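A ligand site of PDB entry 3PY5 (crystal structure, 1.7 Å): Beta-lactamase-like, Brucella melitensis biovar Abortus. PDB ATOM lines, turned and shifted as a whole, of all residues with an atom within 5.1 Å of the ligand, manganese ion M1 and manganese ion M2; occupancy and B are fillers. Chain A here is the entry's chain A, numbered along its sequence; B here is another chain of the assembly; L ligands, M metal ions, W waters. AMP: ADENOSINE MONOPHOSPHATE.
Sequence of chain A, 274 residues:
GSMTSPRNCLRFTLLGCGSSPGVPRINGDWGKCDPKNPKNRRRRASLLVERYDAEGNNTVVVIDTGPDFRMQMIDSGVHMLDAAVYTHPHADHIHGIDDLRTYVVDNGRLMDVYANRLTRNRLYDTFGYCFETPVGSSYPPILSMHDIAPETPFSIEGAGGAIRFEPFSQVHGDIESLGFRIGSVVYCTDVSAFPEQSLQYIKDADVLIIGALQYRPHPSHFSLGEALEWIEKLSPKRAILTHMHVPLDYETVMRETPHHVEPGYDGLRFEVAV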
ATOM      1  N   SER A  20      18.222   0.918 -26.252  1.00  0.00           N
ATOM      2  CA  SER A  20      16.890   1.494 -26.487  1.00  0.00           C
ATOM      3  C   SER A  20      15.723   0.510 -26.794  1.00  0.00           C
ATOM      4  O   SER A  20      14.622   0.793 -26.417  1.00  0.00           O
ATOM      5  CB  SER A  20      16.912   2.612 -27.516  1.00  0.00           C
ATOM      6  OG  SER A  20      17.282   2.136 -28.782  1.00  0.00           O
ATOM      7  N   HIS A  88      18.923  13.321 -21.234  1.00  0.00           N
ATOM      8  CA  HIS A  88      18.776  13.709 -22.637  1.00  0.00           C
ATOM      9  C   HIS A  88      17.389  13.225 -23.139  1.00  0.00           C
ATOM     10  O   HIS A  88      16.812  12.310 -22.529  1.00  0.00           O
ATOM     11  CB  HIS A  88      19.890  13.210 -23.561  1.00  0.00           C
ATOM     12  CG  HIS A  88      19.849  11.732 -23.873  1.00  0.00           C
ATOM     13  ND1 HIS A  88      19.926  10.756 -22.892  1.00  0.00           N
ATOM     14  CD2 HIS A  88      19.837  11.070 -25.056  1.00  0.00           C
ATOM     15  CE1 HIS A  88      19.957   9.570 -23.460  1.00  0.00           C
ATOM     16  NE2 HIS A  88      19.890   9.720 -24.769  1.00  0.00           N
ATOM     17  N   PRO A  89      16.861  13.861 -24.189  1.00  0.00           N
ATOM     18  CA  PRO A  89      15.490  13.553 -24.617  1.00  0.00           C
ATOM     19  C   PRO A  89      15.374  12.520 -25.734  1.00  0.00           C
ATOM     20  O   PRO A  89      15.005  12.867 -26.870  1.00  0.00           O
ATOM     21  CB  PRO A  89      15.003  14.890 -25.154  1.00  0.00           C
ATOM     22  CG  PRO A  89      16.233  15.478 -25.816  1.00  0.00           C
ATOM     23  CD  PRO A  89      17.386  15.073 -24.869  1.00  0.00           C
ATOM     24  N   HIS A  90      15.766  11.306 -25.443  1.00  0.00           N
ATOM     25  CA  HIS A  90      15.548  10.190 -26.332  1.00  0.00           C
ATOM     26  C   HIS A  90      14.458   9.305 -25.702  1.00  0.00           C
ATOM     27  O   HIS A  90      14.329   9.205 -24.477  1.00  0.00           O
ATOM     28  CB  HIS A  90      16.840   9.414 -26.583  1.00  0.00           C
ATOM     29  CG  HIS A  90      17.737  10.040 -27.610  1.00  0.00           C
ATOM     30  ND1 HIS A  90      19.045   9.644 -27.806  1.00  0.00           N
ATOM     31  CD2 HIS A  90      17.524  11.065 -28.492  1.00  0.00           C
ATOM     32  CE1 HIS A  90      19.573  10.348 -28.791  1.00  0.00           C
ATOM     33  NE2 HIS A  90      18.679  11.218 -29.215  1.00  0.00           N
ATOM     34  N   ALA A  91      13.636   8.728 -26.574  1.00  0.00           N
ATOM     35  CA  ALA A  91      12.480   7.884 -26.222  1.00  0.00           C
ATOM     36  C   ALA A  91      12.690   6.974 -24.987  1.00  0.00           C
ATOM     37  O   ALA A  91      11.871   6.926 -24.037  1.00  0.00           O
ATOM     38  CB  ALA A  91      12.134   6.992 -27.460  1.00  0.00           C
ATOM     39  N   ASP A  92      13.778   6.243 -25.026  1.00  0.00           N
ATOM     40  CA  ASP A  92      14.073   5.248 -24.013  1.00  0.00           C
ATOM     41  C   ASP A  92      14.367   5.834 -22.636  1.00  0.00           C
ATOM     42  O   ASP A  92      14.497   5.067 -21.698  1.00  0.00           O
ATOM     43  CB  ASP A  92      15.173   4.271 -24.463  1.00  0.00           C
ATOM     44  CG  ASP A  92      16.450   4.951 -24.955  1.00  0.00           C
ATOM     45  OD1 ASP A  92      16.344   5.929 -25.731  1.00  0.00           O
ATOM     46  OD2 ASP A  92      17.522   4.417 -24.613  1.00  0.00           O
ATOM     47  N   HIS A  93      14.488   7.170 -22.547  1.00  0.00           N
ATOM     48  CA  HIS A  93      14.770   7.897 -21.330  1.00  0.00           C
ATOM     49  C   HIS A  93      13.653   8.820 -20.852  1.00  0.00           C
ATOM     50  O   HIS A  93      13.691   9.314 -19.712  1.00  0.00           O
ATOM     51  CB  HIS A  93      16.116   8.683 -21.524  1.00  0.00           C
ATOM     52  CG  HIS A  93      17.265   7.788 -21.911  1.00  0.00           C
ATOM     53  ND1 HIS A  93      18.217   7.356 -21.002  1.00  0.00           N
ATOM     54  CD2 HIS A  93      17.625   7.290 -23.110  1.00  0.00           C
ATOM     55  CE1 HIS A  93      19.099   6.609 -21.644  1.00  0.00           C
ATOM     56  NE2 HIS A  93      18.771   6.554 -22.929  1.00  0.00           N
ATOM     57  N   ILE A  94      12.604   8.992 -21.656  1.00  0.00           N
ATOM     58  CA  ILE A  94      11.576   9.938 -21.300  1.00  0.00           C
ATOM     59  C   ILE A  94      10.117   9.469 -21.478  1.00  0.00           C
ATOM     60  O   ILE A  94       9.229  10.084 -20.914  1.00  0.00           O
ATOM     61  CB  ILE A  94      11.778  11.281 -22.061  1.00  0.00           C
ATOM     62  CG1 ILE A  94      11.758  11.088 -23.604  1.00  0.00           C
ATOM     63  CG2 ILE A  94      13.046  12.031 -21.526  1.00  0.00           C
ATOM     64  CD1 ILE A  94      11.623  12.411 -24.407  1.00  0.00           C
ATOM     65  N   HIS A  95       9.858   8.417 -22.235  1.00  0.00           N
ATOM     66  CA  HIS A  95       8.494   8.091 -22.612  1.00  0.00           C
ATOM     67  C   HIS A  95       7.628   7.440 -21.507  1.00  0.00           C
ATOM     68  O   HIS A  95       6.454   7.167 -21.729  1.00  0.00           O
ATOM     69  CB  HIS A  95       8.477   7.268 -23.909  1.00  0.00           C
ATOM     70  CG  HIS A  95       8.770   8.072 -25.135  1.00  0.00           C
ATOM     71  ND1 HIS A  95       8.869   7.500 -26.384  1.00  0.00           N
ATOM     72  CD2 HIS A  95       8.982   9.402 -25.314  1.00  0.00           C
ATOM     73  CE1 HIS A  95       9.139   8.441 -27.278  1.00  0.00           C
ATOM     74  NE2 HIS A  95       9.206   9.607 -26.658  1.00  0.00           N
ATOM     75  N   HIS A 172      27.070  12.614 -27.353  1.00  0.00           N
ATOM     76  CA  HIS A 172      26.214  11.470 -27.634  1.00  0.00           C
ATOM     77  C   HIS A 172      25.837  11.494 -29.106  1.00  0.00           C
ATOM     78  O   HIS A 172      24.748  11.891 -29.493  1.00  0.00           O
ATOM     79  CB  HIS A 172      24.978  11.560 -26.734  1.00  0.00           C
ATOM     80  CG  HIS A 172      24.016  10.428 -26.907  1.00  0.00           C
ATOM     81  ND1 HIS A 172      24.411   9.154 -27.254  1.00  0.00           N
ATOM     82  CD2 HIS A 172      22.674  10.378 -26.757  1.00  0.00           C
ATOM     83  CE1 HIS A 172      23.350   8.359 -27.305  1.00  0.00           C
ATOM     84  NE2 HIS A 172      22.289   9.074 -26.996  1.00  0.00           N
ATOM     85  N   ASP A 190      24.720   6.814 -22.500  1.00  0.00           N
ATOM     86  CA  ASP A 190      24.476   7.521 -23.771  1.00  0.00           C
ATOM     87  C   ASP A 190      25.576   8.538 -24.062  1.00  0.00           C
ATOM     88  O   ASP A 190      25.349   9.752 -24.210  1.00  0.00           O
ATOM     89  CB  ASP A 190      23.067   8.132 -23.794  1.00  0.00           C
ATOM     90  CG  ASP A 190      21.975   7.081 -23.767  1.00  0.00           C
ATOM     91  OD1 ASP A 190      21.719   6.488 -22.706  1.00  0.00           O
ATOM     92  OD2 ASP A 190      21.377   6.844 -24.809  1.00  0.00           O
ATOM     93  N   HIS A 218      29.750   2.271 -32.859  1.00  0.00           N
ATOM     94  CA  HIS A 218      28.432   2.859 -33.030  1.00  0.00           C
ATOM     95  C   HIS A 218      28.615   4.344 -32.927  1.00  0.00           C
ATOM     96  O   HIS A 218      29.424   4.811 -32.134  1.00  0.00           O
ATOM     97  CB  HIS A 218      27.469   2.431 -31.935  1.00  0.00           C
ATOM     98  CG  HIS A 218      26.031   2.792 -32.216  1.00  0.00           C
ATOM     99  ND1 HIS A 218      25.519   4.038 -31.946  1.00  0.00           N
ATOM    100  CD2 HIS A 218      25.009   2.065 -32.710  1.00  0.00           C
ATOM    101  CE1 HIS A 218      24.232   4.058 -32.280  1.00  0.00           C
ATOM    102  NE2 HIS A 218      23.904   2.862 -32.736  1.00  0.00           N
ATOM    103  N   SER A 220      26.889   6.679 -31.555  1.00  0.00           N
ATOM    104  CA  SER A 220      26.293   7.354 -30.409  1.00  0.00           C
ATOM    105  C   SER A 220      26.696   6.786 -29.053  1.00  0.00           C
ATOM    106  O   SER A 220      26.266   7.314 -27.980  1.00  0.00           O
ATOM    107  CB  SER A 220      24.772   7.262 -30.502  1.00  0.00           C
ATOM    108  OG  SER A 220      24.310   7.849 -31.703  1.00  0.00           O
ATOM    109  N   HIS A 221      27.417   5.666 -29.054  1.00  0.00           N
ATOM    110  CA  HIS A 221      27.791   5.014 -27.810  1.00  0.00           C
ATOM    111  C   HIS A 221      29.137   4.412 -27.889  1.00  0.00           C
ATOM    112  O   HIS A 221      29.550   3.930 -28.955  1.00  0.00           O
ATOM    113  CB  HIS A 221      26.854   3.868 -27.492  1.00  0.00           C
ATOM    114  CG  HIS A 221      25.403   4.247 -27.455  1.00  0.00           C
ATOM    115  ND1 HIS A 221      24.776   4.634 -26.291  1.00  0.00           N
ATOM    116  CD2 HIS A 221      24.452   4.252 -28.423  1.00  0.00           C
ATOM    117  CE1 HIS A 221      23.509   4.887 -26.550  1.00  0.00           C
ATOM    118  NE2 HIS A 221      23.287   4.681 -27.841  1.00  0.00           N
ATOM    119  N   HIS A 243      23.537   0.279 -20.449  1.00  0.00           N
ATOM    120  CA  HIS A 243      23.037   0.553 -21.811  1.00  0.00           C
ATOM    121  C   HIS A 243      23.544  -0.460 -22.787  1.00  0.00           C
ATOM    122  O   HIS A 243      23.871  -0.112 -23.917  1.00  0.00           O
ATOM    123  CB  HIS A 243      23.345   1.985 -22.268  1.00  0.00           C
ATOM    124  CG  HIS A 243      22.336   2.568 -23.180  1.00  0.00           C
ATOM    125  ND1 HIS A 243      22.247   2.198 -24.506  1.00  0.00           N
ATOM    126  CD2 HIS A 243      21.379   3.512 -22.994  1.00  0.00           C
ATOM    127  CE1 HIS A 243      21.309   2.921 -25.096  1.00  0.00           C
ATOM    128  NE2 HIS A 243      20.739   3.689 -24.190  1.00  0.00           N
ATOM    129  N   ASP B  98       7.489   4.213 -29.820  1.00  0.00           N
ATOM    130  CA  ASP B  98       8.855   4.107 -30.342  1.00  0.00           C
ATOM    131  C   ASP B  98       9.196   2.656 -30.563  1.00  0.00           C
ATOM    132  O   ASP B  98      10.030   2.321 -31.425  1.00  0.00           O
ATOM    133  CB  ASP B  98       9.869   4.720 -29.391  1.00  0.00           C
ATOM    134  CG  ASP B  98      11.228   4.775 -29.992  1.00  0.00           C
ATOM    135  OD1 ASP B  98      11.499   5.691 -30.761  1.00  0.00           O
ATOM    136  OD2 ASP B  98      12.017   3.873 -29.697  1.00  0.00           O
ATOM    137  N   ARG B 101       9.781   0.430 -33.776  1.00  0.00           N
ATOM    138  CA  ARG B 101      10.968   0.515 -34.636  1.00  0.00           C
ATOM    139  C   ARG B 101      11.510  -0.842 -35.060  1.00  0.00           C
ATOM    140  O   ARG B 101      11.886  -1.003 -36.223  1.00  0.00           O
ATOM    141  CB  ARG B 101      12.076   1.281 -33.889  1.00  0.00           C
ATOM    142  CG  ARG B 101      13.351   1.526 -34.674  1.00  0.00           C
ATOM    143  CD  ARG B 101      14.271   2.348 -33.762  1.00  0.00           C
ATOM    144  NE  ARG B 101      13.545   3.560 -33.386  1.00  0.00           N
ATOM    145  CZ  ARG B 101      13.427   4.632 -34.175  1.00  0.00           C
ATOM    146  NH1 ARG B 101      14.025   4.650 -35.358  1.00  0.00           N
ATOM    147  NH2 ARG B 101      12.709   5.693 -33.785  1.00  0.00           N
ATOM    148  N   TYR B 129       9.239  12.860 -34.766  1.00  0.00           N
ATOM    149  CA  TYR B 129      10.392  12.142 -35.294  1.00  0.00           C
ATOM    150  C   TYR B 129      10.061  10.757 -35.873  1.00  0.00           C
ATOM    151  O   TYR B 129      10.842  10.174 -36.637  1.00  0.00           O
ATOM    152  CB  TYR B 129      11.481  12.024 -34.220  1.00  0.00           C
ATOM    153  CG  TYR B 129      11.157  10.976 -33.195  1.00  0.00           C
ATOM    154  CD1 TYR B 129      10.298  11.247 -32.145  1.00  0.00           C
ATOM    155  CD2 TYR B 129      11.725   9.724 -33.271  1.00  0.00           C
ATOM    156  CE1 TYR B 129      10.005  10.273 -31.224  1.00  0.00           C
ATOM    157  CE2 TYR B 129      11.431   8.758 -32.354  1.00  0.00           C
ATOM    158  CZ  TYR B 129      10.581   9.022 -31.320  1.00  0.00           C
ATOM    159  OH  TYR B 129      10.290   8.000 -30.449  1.00  0.00           O
ATOM    160  N   PRO B 134      13.666  15.283 -37.881  1.00  0.00           N
ATOM    161  CA  PRO B 134      13.818  16.687 -37.536  1.00  0.00           C
ATOM    162  C   PRO B 134      15.187  17.252 -37.811  1.00  0.00           C
ATOM    163  O   PRO B 134      16.175  16.494 -37.993  1.00  0.00           O
ATOM    164  CB  PRO B 134      13.590  16.713 -36.030  1.00  0.00           C
ATOM    165  CG  PRO B 134      14.061  15.425 -35.548  1.00  0.00           C
ATOM    166  CD  PRO B 134      13.728  14.421 -36.678  1.00  0.00           C
ATOM    167  N   SER B 137      19.076  15.666 -36.897  1.00  0.00           N
ATOM    168  CA  SER B 137      18.961  14.206 -36.639  1.00  0.00           C
ATOM    169  C   SER B 137      19.277  13.399 -37.880  1.00  0.00           C
ATOM    170  O   SER B 137      19.098  13.848 -39.006  1.00  0.00           O
ATOM    171  CB  SER B 137      17.540  13.865 -36.163  1.00  0.00           C
ATOM    172  OG  SER B 137      17.375  12.452 -35.980  1.00  0.00           O
ATOM    173  N   TYR B 139      18.035  10.030 -37.735  1.00  0.00           N
ATOM    174  CA  TYR B 139      17.114   8.903 -37.602  1.00  0.00           C
ATOM    175  C   TYR B 139      16.032   8.980 -38.690  1.00  0.00           C
ATOM    176  O   TYR B 139      15.283   9.967 -38.765  1.00  0.00           O
ATOM    177  CB  TYR B 139      16.479   8.876 -36.188  1.00  0.00           C
ATOM    178  CG  TYR B 139      17.417   8.398 -35.105  1.00  0.00           C
ATOM    179  CD1 TYR B 139      17.634   7.050 -34.887  1.00  0.00           C
ATOM    180  CD2 TYR B 139      18.083   9.286 -34.280  1.00  0.00           C
ATOM    181  CE1 TYR B 139      18.495   6.599 -33.909  1.00  0.00           C
ATOM    182  CE2 TYR B 139      18.949   8.844 -33.266  1.00  0.00           C
ATOM    183  CZ  TYR B 139      19.150   7.503 -33.097  1.00  0.00           C
ATOM    184  OH  TYR B 139      19.978   7.015 -32.121  1.00  0.00           O
HETATM  185  P   AMP L   1      20.034   5.484 -28.071  1.00  0.00           P
HETATM  186  O1P AMP L   1      20.640   6.909 -28.074  1.00  0.00           O
HETATM  187  O2P AMP L   1      20.705   4.505 -29.033  1.00  0.00           O
HETATM  188  O3P AMP L   1      19.958   4.771 -26.729  1.00  0.00           O
HETATM  189  O5' AMP L   1      18.509   5.479 -28.627  1.00  0.00           O
HETATM  190  C5' AMP L   1      17.858   6.482 -29.385  1.00  0.00           C
HETATM  191  C4' AMP L   1      16.383   6.335 -29.005  1.00  0.00           C
HETATM  192  O4' AMP L   1      15.735   7.587 -29.197  1.00  0.00           O
HETATM  193  C3' AMP L   1      15.602   5.319 -29.835  1.00  0.00           C
HETATM  194  O3' AMP L   1      14.497   4.906 -29.036  1.00  0.00           O
HETATM  195  C2' AMP L   1      15.085   6.174 -30.969  1.00  0.00           C
HETATM  196  O2' AMP L   1      13.971   5.583 -31.640  1.00  0.00           O
HETATM  197  C1' AMP L   1      14.737   7.423 -30.199  1.00  0.00           C
HETATM  198  N9  AMP L   1      14.707   8.695 -30.946  1.00  0.00           N
HETATM  199  C8  AMP L   1      15.201   8.937 -32.180  1.00  0.00           C
HETATM  200  N7  AMP L   1      14.986  10.223 -32.517  1.00  0.00           N
HETATM  201  C5  AMP L   1      14.331  10.800 -31.483  1.00  0.00           C
HETATM  202  C6  AMP L   1      13.776  12.135 -31.228  1.00  0.00           C
HETATM  203  N6  AMP L   1      13.878  13.159 -32.106  1.00  0.00           N
HETATM  204  N1  AMP L   1      13.173  12.293 -30.031  1.00  0.00           N
HETATM  205  C2  AMP L   1      13.044  11.282 -29.124  1.00  0.00           C
HETATM  206  N3  AMP L   1      13.505  10.035 -29.299  1.00  0.00           N
HETATM  207  C4  AMP L   1      14.158   9.769 -30.455  1.00  0.00           C
HETATM  208 MN    MN M   1      19.554   5.489 -24.666  1.00  0.00          MN
HETATM  209 MN    MN M   2      20.203   8.259 -26.461  1.00  0.00          MN
HETATM  210  O   HOH W   1      12.660   3.064 -26.868  1.00  0.00           O
HETATM  211  O   HOH W   2      18.770   6.978 -25.986  1.00  0.00           O
HETATM  212  O   HOH W   3      20.029   4.357 -31.608  1.00  0.00           O
HETATM  213  O   HOH W   4      20.194   1.882 -28.195  1.00  0.00           O
HETATM  214  O   HOH W   5      13.003  15.580 -32.031  1.00  0.00           O
HETATM  215  O   HOH W   6      21.612   7.814 -30.253  1.00  0.00           O
HETATM  216  O   HOH W   7      10.612  14.091 -30.040  1.00  0.00           O
HETATM  217  O   HOH W   8      15.126  11.910 -34.933  1.00  0.00           O
HETATM  218  O   HOH W   9      12.583  14.774 -27.892  1.00  0.00           O
HETATM  219  O   HOH W  10      15.250  14.647 -29.147  1.00  0.00           O
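Four residues have an atom within 4 Å of manganese ion M2: His 88, His 90, His 172 and Asp 190.
Merely in contact with the ligand: Ser 20 (3.5 Å), Pro 89 (3.4 Å), Tyr 129 of chain B (3.3 Å) and Tyr 139 of chain B (3.5 Å).
Hydrophobic or aromatic side chains that line the ligand: His 90, Ala 91, His 172, His 221, His 243, Tyr 129 of chain B and Tyr 139 of chain B.
The nearest printed residue that does not touch the ligand is Pro 134 of chain B (4.1 Å).
The guanidinium group (NH2) of Arg 101 of chain B is in hydrogen-bond range of an oxygen (O2') of the ligand.
The side-chain carboxylate of Asp 98 of chain B sits at hydrogen-bond distance from an oxygen (O2') of the ligand (2.6 Å).
NE2 of His 221 is in hydrogen-bond range of O2P of the ligand (2.8 Å).
N of Ala 91 sits at hydrogen-bond distance from N3 of the ligand (3.0 Å).
Water W2 is bound to manganese ion M2.
Manganese ion M2 is bound by O1P of the ligand, 2.1 Å away.
ND1 of His 90 binds manganese ion M2 (2.3 Å).
A ring nitrogen (NE2) of His 88 is bound to manganese ion M2 (2.3 Å).
Manganese ion M2 is bound by NE2 of His 172, at 2.3 Å.
Manganese ion M2 is bound by OD2 of Asp 190 (2.5 Å).
Manganese ion M1 is bound by water W2, NE2 of His 93, NE2 of His 243, O3P of the ligand, OD2 of Asp 190 and OD2 of Asp 92.
Manganese ion M1 has six donor atoms within binding distance.
A ring nitrogen (ND1) of His 172 is in hydrogen-bond range of the backbone carbonyl oxygen (O) of Ser 220, 2.7 Å away.
NH2 of Arg 101 of chain B lies within salt-bridge range of OD1 of Asp 98 of chain B (3.3 Å).
The side-chain hydroxyl (OH) of Tyr 129 of chain B lies within hydrogen-bond range of the side-chain carboxylate (OD1) of Asp 98 of chain B (2.6 Å).
The backbone NH of Tyr 139 of chain B sits at hydrogen-bond distance from the side-chain hydroxyl of Ser 137 of chain B, 3.1 Å away.
Within 4 Å of manganese ion M1: Asp 92, His 93, Asp 190 and His 243.
Water W2 bridges OD1 of Asp 92 (2.7 Å) and O5' of the ligand (3.0 Å).
Water W6 bridges the side-chain hydroxyl of Tyr 139 of chain B and the side-chain hydroxyl of Ser 220.
Water W4 bridges an oxygen (O2P) of the ligand (2.8 Å) and the backbone NH of Ser 20 (2.9 Å).
Water W8 bridges OG of Ser 137 of chain B (2.5 Å) and N7 of the ligand (3.0 Å).
Water W10 lies within hydrogen-bond range of the backbone carbonyl oxygen of Pro 89 (2.9 Å) and a nitrogen (N1) of the ligand (3.3 Å).
Water W9 lies within hydrogen-bond range of the backbone carbonyl oxygen (O) of Pro 89 (3.2 Å) and a nitrogen (N1) of the ligand (3.3 Å).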
